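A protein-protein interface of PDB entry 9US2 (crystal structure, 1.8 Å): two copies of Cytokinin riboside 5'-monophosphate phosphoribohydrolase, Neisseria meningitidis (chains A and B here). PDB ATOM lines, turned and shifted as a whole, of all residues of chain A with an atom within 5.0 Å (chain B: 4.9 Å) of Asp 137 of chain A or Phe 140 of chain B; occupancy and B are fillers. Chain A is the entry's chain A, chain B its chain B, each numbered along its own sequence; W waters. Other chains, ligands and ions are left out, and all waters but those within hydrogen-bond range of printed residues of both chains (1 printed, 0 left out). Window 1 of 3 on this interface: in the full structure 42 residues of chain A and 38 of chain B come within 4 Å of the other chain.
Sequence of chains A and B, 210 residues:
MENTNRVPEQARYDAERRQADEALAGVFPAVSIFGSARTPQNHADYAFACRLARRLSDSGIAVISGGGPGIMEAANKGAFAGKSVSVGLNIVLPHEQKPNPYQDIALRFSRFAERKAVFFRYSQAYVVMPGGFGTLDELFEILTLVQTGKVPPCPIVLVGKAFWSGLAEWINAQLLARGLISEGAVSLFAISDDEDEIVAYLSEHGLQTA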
ATOM      1  N   LYS A 116      17.838 -14.719   9.543  1.00  0.00           N
ATOM      2  CA  LYS A 116      18.206 -15.330  10.816  1.00  0.00           C
ATOM      3  C   LYS A 116      16.980 -15.614  11.677  1.00  0.00           C
ATOM      4  O   LYS A 116      16.932 -16.638  12.382  1.00  0.00           O
ATOM      5  CB  LYS A 116      19.209 -14.423  11.545  1.00  0.00           C
ATOM      6  CG  LYS A 116      20.646 -14.567  11.017  1.00  0.00           C
ATOM      7  CD  LYS A 116      21.606 -13.624  11.782  1.00  0.00           C
ATOM      8  CE  LYS A 116      21.496 -12.188  11.254  1.00  0.00           C
ATOM      9  NZ  LYS A 116      22.343 -11.219  12.008  1.00  0.00           N
ATOM     10  N   PHE A 133      33.033 -14.295   8.830  1.00  0.00           N
ATOM     11  CA  PHE A 133      32.402 -13.335   9.732  1.00  0.00           C
ATOM     12  C   PHE A 133      30.892 -13.536   9.800  1.00  0.00           C
ATOM     13  O   PHE A 133      30.280 -13.339  10.859  1.00  0.00           O
ATOM     14  CB  PHE A 133      32.717 -11.893   9.300  1.00  0.00           C
ATOM     15  CG  PHE A 133      34.154 -11.471   9.525  1.00  0.00           C
ATOM     16  CD1 PHE A 133      34.959 -12.121  10.451  1.00  0.00           C
ATOM     17  CD2 PHE A 133      34.691 -10.395   8.811  1.00  0.00           C
ATOM     18  CE1 PHE A 133      36.290 -11.710  10.656  1.00  0.00           C
ATOM     19  CE2 PHE A 133      36.002  -9.976   9.021  1.00  0.00           C
ATOM     20  CZ  PHE A 133      36.803 -10.636   9.946  1.00  0.00           C
ATOM     21  N   GLY A 134      30.262 -13.876   8.677  1.00  0.00           N
ATOM     22  CA  GLY A 134      28.821 -14.086   8.692  1.00  0.00           C
ATOM     23  C   GLY A 134      28.449 -15.330   9.468  1.00  0.00           C
ATOM     24  O   GLY A 134      27.412 -15.366  10.144  1.00  0.00           O
ATOM     25  N   THR A 135      29.301 -16.353   9.408  1.00  0.00           N
ATOM     26  CA  THR A 135      29.116 -17.528  10.263  1.00  0.00           C
ATOM     27  C   THR A 135      29.270 -17.182  11.744  1.00  0.00           C
ATOM     28  O   THR A 135      28.518 -17.691  12.589  1.00  0.00           O
ATOM     29  CB  THR A 135      30.102 -18.625   9.853  1.00  0.00           C
ATOM     30  OG1 THR A 135      29.855 -19.003   8.485  1.00  0.00           O
ATOM     31  CG2 THR A 135      29.955 -19.858  10.770  1.00  0.00           C
ATOM     32  N   LEU A 136      30.240 -16.327  12.090  1.00  0.00           N
ATOM     33  CA  LEU A 136      30.427 -15.951  13.492  1.00  0.00           C
ATOM     34  C   LEU A 136      29.305 -15.037  13.986  1.00  0.00           C
ATOM     35  O   LEU A 136      28.931 -15.083  15.165  1.00  0.00           O
ATOM     36  CB  LEU A 136      31.792 -15.290  13.657  1.00  0.00           C
ATOM     37  CG  LEU A 136      32.964 -16.245  13.380  1.00  0.00           C
ATOM     38  CD1 LEU A 136      34.275 -15.494  13.397  1.00  0.00           C
ATOM     39  CD2 LEU A 136      32.982 -17.451  14.372  1.00  0.00           C
ATOM     40  N   ASP A 137      28.750 -14.215  13.097  1.00  0.00           N
ATOM     41  CA  ASP A 137      27.526 -13.488  13.423  1.00  0.00           C
ATOM     42  C   ASP A 137      26.429 -14.459  13.852  1.00  0.00           C
ATOM     43  O   ASP A 137      25.834 -14.314  14.930  1.00  0.00           O
ATOM     44  CB  ASP A 137      27.117 -12.657  12.202  1.00  0.00           C
ATOM     45  CG  ASP A 137      25.754 -11.989  12.340  1.00  0.00           C
ATOM     46  OD1 ASP A 137      25.372 -11.642  13.474  1.00  0.00           O
ATOM     47  OD2 ASP A 137      25.085 -11.788  11.283  1.00  0.00           O
ATOM     48  N   GLU A 138      26.184 -15.488  13.044  1.00  0.00           N
ATOM     49  CA  GLU A 138      25.156 -16.472  13.395  1.00  0.00           C
ATOM     50  C   GLU A 138      25.469 -17.169  14.707  1.00  0.00           C
ATOM     51  O   GLU A 138      24.579 -17.341  15.561  1.00  0.00           O
ATOM     52  CB  GLU A 138      25.016 -17.494  12.270  1.00  0.00           C
ATOM     53  CG  GLU A 138      24.409 -16.863  11.012  1.00  0.00           C
ATOM     54  CD  GLU A 138      24.527 -17.707   9.754  1.00  0.00           C
ATOM     55  OE1 GLU A 138      25.520 -18.446   9.594  1.00  0.00           O
ATOM     56  OE2 GLU A 138      23.596 -17.613   8.903  1.00  0.00           O
ATOM     57  N   LEU A 139      26.723 -17.585  14.878  1.00  0.00           N
ATOM     58  CA  LEU A 139      27.130 -18.308  16.079  1.00  0.00           C
ATOM     59  C   LEU A 139      26.922 -17.466  17.334  1.00  0.00           C
ATOM     60  O   LEU A 139      26.284 -17.903  18.298  1.00  0.00           O
ATOM     61  CB  LEU A 139      28.598 -18.732  15.941  1.00  0.00           C
ATOM     62  CG  LEU A 139      29.207 -19.337  17.210  1.00  0.00           C
ATOM     63  CD1 LEU A 139      28.334 -20.513  17.713  1.00  0.00           C
ATOM     64  CD2 LEU A 139      30.683 -19.765  17.019  1.00  0.00           C
ATOM     65  N   PHE A 140      27.475 -16.258  17.365  1.00  0.00           N
ATOM     66  CA  PHE A 140      27.330 -15.510  18.607  1.00  0.00           C
ATOM     67  C   PHE A 140      25.928 -14.950  18.785  1.00  0.00           C
ATOM     68  O   PHE A 140      25.521 -14.699  19.919  1.00  0.00           O
ATOM     69  CB  PHE A 140      28.402 -14.412  18.696  1.00  0.00           C
ATOM     70  CG  PHE A 140      29.767 -14.974  18.953  1.00  0.00           C
ATOM     71  CD1 PHE A 140      30.031 -15.627  20.154  1.00  0.00           C
ATOM     72  CD2 PHE A 140      30.750 -14.939  17.981  1.00  0.00           C
ATOM     73  CE1 PHE A 140      31.271 -16.190  20.402  1.00  0.00           C
ATOM     74  CE2 PHE A 140      32.014 -15.505  18.217  1.00  0.00           C
ATOM     75  CZ  PHE A 140      32.257 -16.154  19.437  1.00  0.00           C
ATOM     76  N   GLU A 141      25.177 -14.762  17.701  1.00  0.00           N
ATOM     77  CA  GLU A 141      23.776 -14.361  17.844  1.00  0.00           C
ATOM     78  C   GLU A 141      22.948 -15.468  18.482  1.00  0.00           C
ATOM     79  O   GLU A 141      22.218 -15.222  19.446  1.00  0.00           O
ATOM     80  CB  GLU A 141      23.176 -13.967  16.489  1.00  0.00           C
ATOM     81  CG  GLU A 141      21.848 -13.199  16.630  1.00  0.00           C
ATOM     82  CD  GLU A 141      21.461 -12.438  15.370  1.00  0.00           C
ATOM     83  OE1 GLU A 141      22.350 -11.800  14.751  1.00  0.00           O
ATOM     84  OE2 GLU A 141      20.252 -12.469  15.002  1.00  0.00           O
ATOM     85  N   ILE A 142      23.068 -16.704  17.994  1.00  0.00           N
ATOM     86  CA  ILE A 142      22.265 -17.760  18.614  1.00  0.00           C
ATOM     87  C   ILE A 142      22.728 -18.027  20.053  1.00  0.00           C
ATOM     88  O   ILE A 142      21.904 -18.270  20.936  1.00  0.00           O
ATOM     89  CB  ILE A 142      22.255 -19.043  17.760  1.00  0.00           C
ATOM     90  CG1 ILE A 142      21.228 -20.057  18.319  1.00  0.00           C
ATOM     91  CG2 ILE A 142      23.652 -19.689  17.658  1.00  0.00           C
ATOM     92  CD1 ILE A 142      19.814 -19.502  18.479  1.00  0.00           C
ATOM     93  N   LEU B 136      30.101  -9.816  20.975  1.00  0.00           N
ATOM     94  CA  LEU B 136      30.634 -10.474  19.776  1.00  0.00           C
ATOM     95  C   LEU B 136      29.571 -10.627  18.689  1.00  0.00           C
ATOM     96  O   LEU B 136      29.897 -10.573  17.503  1.00  0.00           O
ATOM     97  CB  LEU B 136      31.210 -11.836  20.144  1.00  0.00           C
ATOM     98  CG  LEU B 136      32.367 -11.714  21.138  1.00  0.00           C
ATOM     99  CD1 LEU B 136      32.808 -13.108  21.573  1.00  0.00           C
ATOM    100  CD2 LEU B 136      33.540 -10.910  20.547  1.00  0.00           C
ATOM    101  N   ASP B 137      28.307 -10.840  19.073  1.00  0.00           N
ATOM    102  CA  ASP B 137      27.206 -10.783  18.106  1.00  0.00           C
ATOM    103  C   ASP B 137      27.206  -9.441  17.378  1.00  0.00           C
ATOM    104  O   ASP B 137      27.271  -9.386  16.144  1.00  0.00           O
ATOM    105  CB  ASP B 137      25.877 -11.021  18.839  1.00  0.00           C
ATOM    106  CG  ASP B 137      24.638 -10.774  17.946  1.00  0.00           C
ATOM    107  OD1 ASP B 137      24.737 -10.885  16.702  1.00  0.00           O
ATOM    108  OD2 ASP B 137      23.569 -10.437  18.513  1.00  0.00           O
ATOM    109  N   GLU B 138      27.212  -8.345  18.134  1.00  0.00           N
ATOM    110  CA  GLU B 138      27.279  -7.005  17.537  1.00  0.00           C
ATOM    111  C   GLU B 138      28.498  -6.824  16.629  1.00  0.00           C
ATOM    112  O   GLU B 138      28.389  -6.278  15.519  1.00  0.00           O
ATOM    113  CB  GLU B 138      27.287  -5.943  18.647  1.00  0.00           C
ATOM    114  CG  GLU B 138      25.923  -5.758  19.309  1.00  0.00           C
ATOM    115  CD  GLU B 138      25.983  -5.118  20.707  1.00  0.00           C
ATOM    116  OE1 GLU B 138      27.068  -5.056  21.323  1.00  0.00           O
ATOM    117  OE2 GLU B 138      24.916  -4.673  21.190  1.00  0.00           O
ATOM    118  N   LEU B 139      29.672  -7.266  17.092  1.00  0.00           N
ATOM    119  CA  LEU B 139      30.910  -7.068  16.342  1.00  0.00           C
ATOM    120  C   LEU B 139      30.884  -7.808  15.012  1.00  0.00           C
ATOM    121  O   LEU B 139      31.128  -7.217  13.955  1.00  0.00           O
ATOM    122  CB  LEU B 139      32.114  -7.532  17.183  1.00  0.00           C
ATOM    123  CG  LEU B 139      33.453  -7.558  16.411  1.00  0.00           C
ATOM    124  CD1 LEU B 139      33.753  -6.204  15.768  1.00  0.00           C
ATOM    125  CD2 LEU B 139      34.612  -7.999  17.333  1.00  0.00           C
ATOM    126  N   PHE B 140      30.631  -9.116  15.043  1.00  0.00           N
ATOM    127  CA  PHE B 140      30.629  -9.861  13.790  1.00  0.00           C
ATOM    128  C   PHE B 140      29.434  -9.502  12.916  1.00  0.00           C
ATOM    129  O   PHE B 140      29.529  -9.618  11.695  1.00  0.00           O
ATOM    130  CB  PHE B 140      30.712 -11.365  14.090  1.00  0.00           C
ATOM    131  CG  PHE B 140      32.076 -11.761  14.544  1.00  0.00           C
ATOM    132  CD1 PHE B 140      33.170 -11.574  13.696  1.00  0.00           C
ATOM    133  CD2 PHE B 140      32.296 -12.171  15.839  1.00  0.00           C
ATOM    134  CE1 PHE B 140      34.455 -11.879  14.119  1.00  0.00           C
ATOM    135  CE2 PHE B 140      33.589 -12.474  16.281  1.00  0.00           C
ATOM    136  CZ  PHE B 140      34.666 -12.323  15.420  1.00  0.00           C
ATOM    137  N   GLU B 141      28.346  -8.987  13.509  1.00  0.00           N
ATOM    138  CA  GLU B 141      27.237  -8.520  12.688  1.00  0.00           C
ATOM    139  C   GLU B 141      27.629  -7.277  11.899  1.00  0.00           C
ATOM    140  O   GLU B 141      27.370  -7.197  10.692  1.00  0.00           O
ATOM    141  CB  GLU B 141      25.993  -8.250  13.541  1.00  0.00           C
ATOM    142  CG  GLU B 141      24.718  -8.114  12.655  1.00  0.00           C
ATOM    143  CD  GLU B 141      23.414  -8.249  13.432  1.00  0.00           C
ATOM    144  OE1 GLU B 141      23.356  -9.085  14.349  1.00  0.00           O
ATOM    145  OE2 GLU B 141      22.440  -7.532  13.094  1.00  0.00           O
ATOM    146  N   ILE B 142      28.291  -6.310  12.539  1.00  0.00           N
ATOM    147  CA  ILE B 142      28.636  -5.108  11.776  1.00  0.00           C
ATOM    148  C   ILE B 142      29.703  -5.428  10.740  1.00  0.00           C
ATOM    149  O   ILE B 142      29.648  -4.937   9.602  1.00  0.00           O
ATOM    150  CB  ILE B 142      29.033  -3.931  12.696  1.00  0.00           C
ATOM    151  CG1 ILE B 142      29.218  -2.649  11.866  1.00  0.00           C
ATOM    152  CG2 ILE B 142      30.307  -4.196  13.535  1.00  0.00           C
ATOM    153  CD1 ILE B 142      27.970  -2.169  11.182  1.00  0.00           C
ATOM    154  N   LEU B 143      30.663  -6.288  11.087  1.00  0.00           N
ATOM    155  CA  LEU B 143      31.653  -6.706  10.098  1.00  0.00           C
ATOM    156  C   LEU B 143      30.982  -7.375   8.902  1.00  0.00           C
ATOM    157  O   LEU B 143      31.326  -7.091   7.751  1.00  0.00           O
ATOM    158  CB  LEU B 143      32.672  -7.641  10.737  1.00  0.00           C
ATOM    159  CG  LEU B 143      33.591  -6.976  11.753  1.00  0.00           C
ATOM    160  CD1 LEU B 143      34.344  -8.035  12.557  1.00  0.00           C
ATOM    161  CD2 LEU B 143      34.561  -6.064  11.017  1.00  0.00           C
ATOM    162  N   THR B 144      29.994  -8.237   9.153  1.00  0.00           N
ATOM    163  CA  THR B 144      29.275  -8.886   8.058  1.00  0.00           C
ATOM    164  C   THR B 144      28.505  -7.871   7.222  1.00  0.00           C
ATOM    165  O   THR B 144      28.567  -7.896   5.986  1.00  0.00           O
ATOM    166  CB  THR B 144      28.345  -9.958   8.612  1.00  0.00           C
ATOM    167  OG1 THR B 144      29.148 -10.939   9.273  1.00  0.00           O
ATOM    168  CG2 THR B 144      27.522 -10.651   7.494  1.00  0.00           C
ATOM    169  N   LEU B 167      41.928 -13.141  19.467  1.00  0.00           N
ATOM    170  CA  LEU B 167      40.895 -13.307  18.451  1.00  0.00           C
ATOM    171  C   LEU B 167      41.411 -12.899  17.078  1.00  0.00           C
ATOM    172  O   LEU B 167      41.180 -13.600  16.086  1.00  0.00           O
ATOM    173  CB  LEU B 167      39.655 -12.497  18.837  1.00  0.00           C
ATOM    174  CG  LEU B 167      38.488 -12.549  17.853  1.00  0.00           C
ATOM    175  CD1 LEU B 167      37.955 -13.974  17.816  1.00  0.00           C
ATOM    176  CD2 LEU B 167      37.378 -11.596  18.324  1.00  0.00           C
ATOM    177  N   ILE B 171      41.659 -15.201  13.751  1.00  0.00           N
ATOM    178  CA  ILE B 171      41.060 -14.780  12.481  1.00  0.00           C
ATOM    179  C   ILE B 171      42.100 -14.810  11.364  1.00  0.00           C
ATOM    180  O   ILE B 171      41.832 -15.287  10.255  1.00  0.00           O
ATOM    181  CB  ILE B 171      40.432 -13.380  12.624  1.00  0.00           C
ATOM    182  CG1 ILE B 171      39.154 -13.425  13.475  1.00  0.00           C
ATOM    183  CG2 ILE B 171      40.151 -12.770  11.263  1.00  0.00           C
ATOM    184  CD1 ILE B 171      38.719 -12.036  13.982  1.00  0.00           C
HETATM  185  O   HOH W   1      21.892  -8.690  10.544  1.00  0.00           O
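OE1 of Glu 141 of chain A sits close to OD1 of Asp 137 of chain B (3.2 Å). The side-chain carboxylate of Asp 137 of chain A lies close to the side-chain carboxylate of Asp 137 of chain B (3.4 Å). The side-chain hydroxyl (OG1) of Thr 144 of chain B lies within hydrogen-bond range of the backbone carbonyl oxygen (O) of Phe 133 of chain A. The side-chain amino group (NZ) of Lys 116 of chain A lies within salt-bridge range of the side-chain carboxylate (OE1) of Glu 141 of chain B (3.3 Å). OE1 of Glu 141 of chain B sits close to OE1 of Glu 141 of chain A, at 2.9 Å. The side-chain hydroxyl of Thr 144 of chain B sits at hydrogen-bond distance from the backbone NH of Gly 134 of chain A (3.2 Å). OD1 of Asp 137 of chain A sits close to OE1 of Glu 141 of chain B, 3.4 Å away.
Phe 140 of chain B touches Phe 133 of chain A. CD2 of Phe 133 of chain A touches CB of Leu 143 of chain B, 3.9 Å away. CB of Leu 136 of chain A touches CG of Phe 140 of chain B, 3.6 Å away. N of Asp 137 of chain A touches CB of Phe 140 of chain B, 3.6 Å away. Asp 137 of chain A touches Thr 144 of chain B (CB to OG1, 3.96 Å). CE1 of Phe 140 of chain A touches CD1 of Leu 136 of chain B, 3.6 Å away. Asp 137 of chain B touches Phe 140 of chain A (N to CB, 3.6 Å). Phe 140 of chain A touches Phe 140 of chain B.
Asp 137 of chain A touches just these residues of chain B: Asp 137, Phe 140, Glu 141 and Thr 144. Of chain A, only Phe 133, Leu 136, Asp 137 and Phe 140 come within 4 Å of Phe 140 of chain B. Printed residues of chain B within 4 Å of Gly 134 of chain A: Thr 144 (3.2 Å). Of the printed residues of chain A, Glu 141 of chain B touches Lys 116, Asp 137 and Glu 141. Glu 138 of chain B touches none of the printed residues of chain A. The nearest printed residue of chain B that does not touch Asp 137 of chain A is Leu 136 of chain B (5.5 Å). The nearest printed residue of chain B that does not touch Leu 136 of chain A is Leu 136 of chain B (5.2 Å).
Leu 136 of chain A touches Phe 140 of chain B, and with the chains exchanged Phe 140 of chain A touches Leu 136 of chain B. Asp 137 of chain A touches its own counterpart, Asp 137 of chain B. Asp 137 of chain A touches Glu 141 of chain B, and with the chains exchanged Glu 141 of chain A touches Asp 137 of chain B. Phe 140 of chain B touches its own counterpart, Phe 140 of chain A.
Of the 11 printed residues of chain B, 6 touch a printed residue of chain A. Hydrophobic or aromatic side chains of chain A within 4 Å of the printed part of chain B: Phe 133, Leu 136 and Phe 140. Among the printed residues, Asp or Glu carboxylates within 4 Å of a Lys or Arg side-chain nitrogen of the other chain: Lys 116 of chain A with Glu 141 of chain B (3.3 Å).
Water W1 lies within hydrogen-bond range of the side-chain carboxylate (OE2) of Glu 141 of chain B (2.9 Å) and the side-chain amino group (NZ) of Lys 116 of chain A (3.0 Å).
The side-chain carboxylate (OE1) of Glu 141 of chain A is in salt-bridge range of the side-chain amino group (NZ) of Lys 116 of chain A, 2.8 Å away. The side-chain amino group (NZ) of Lys 116 of chain A lies within salt-bridge range of the side-chain carboxylate (OD2) of Asp 137 of chain A. The side-chain hydroxyl (OG1) of Thr 144 of chain B sits at hydrogen-bond distance from the backbone carbonyl oxygen (O) of Phe 140 of chain B, 2.8 Å away.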
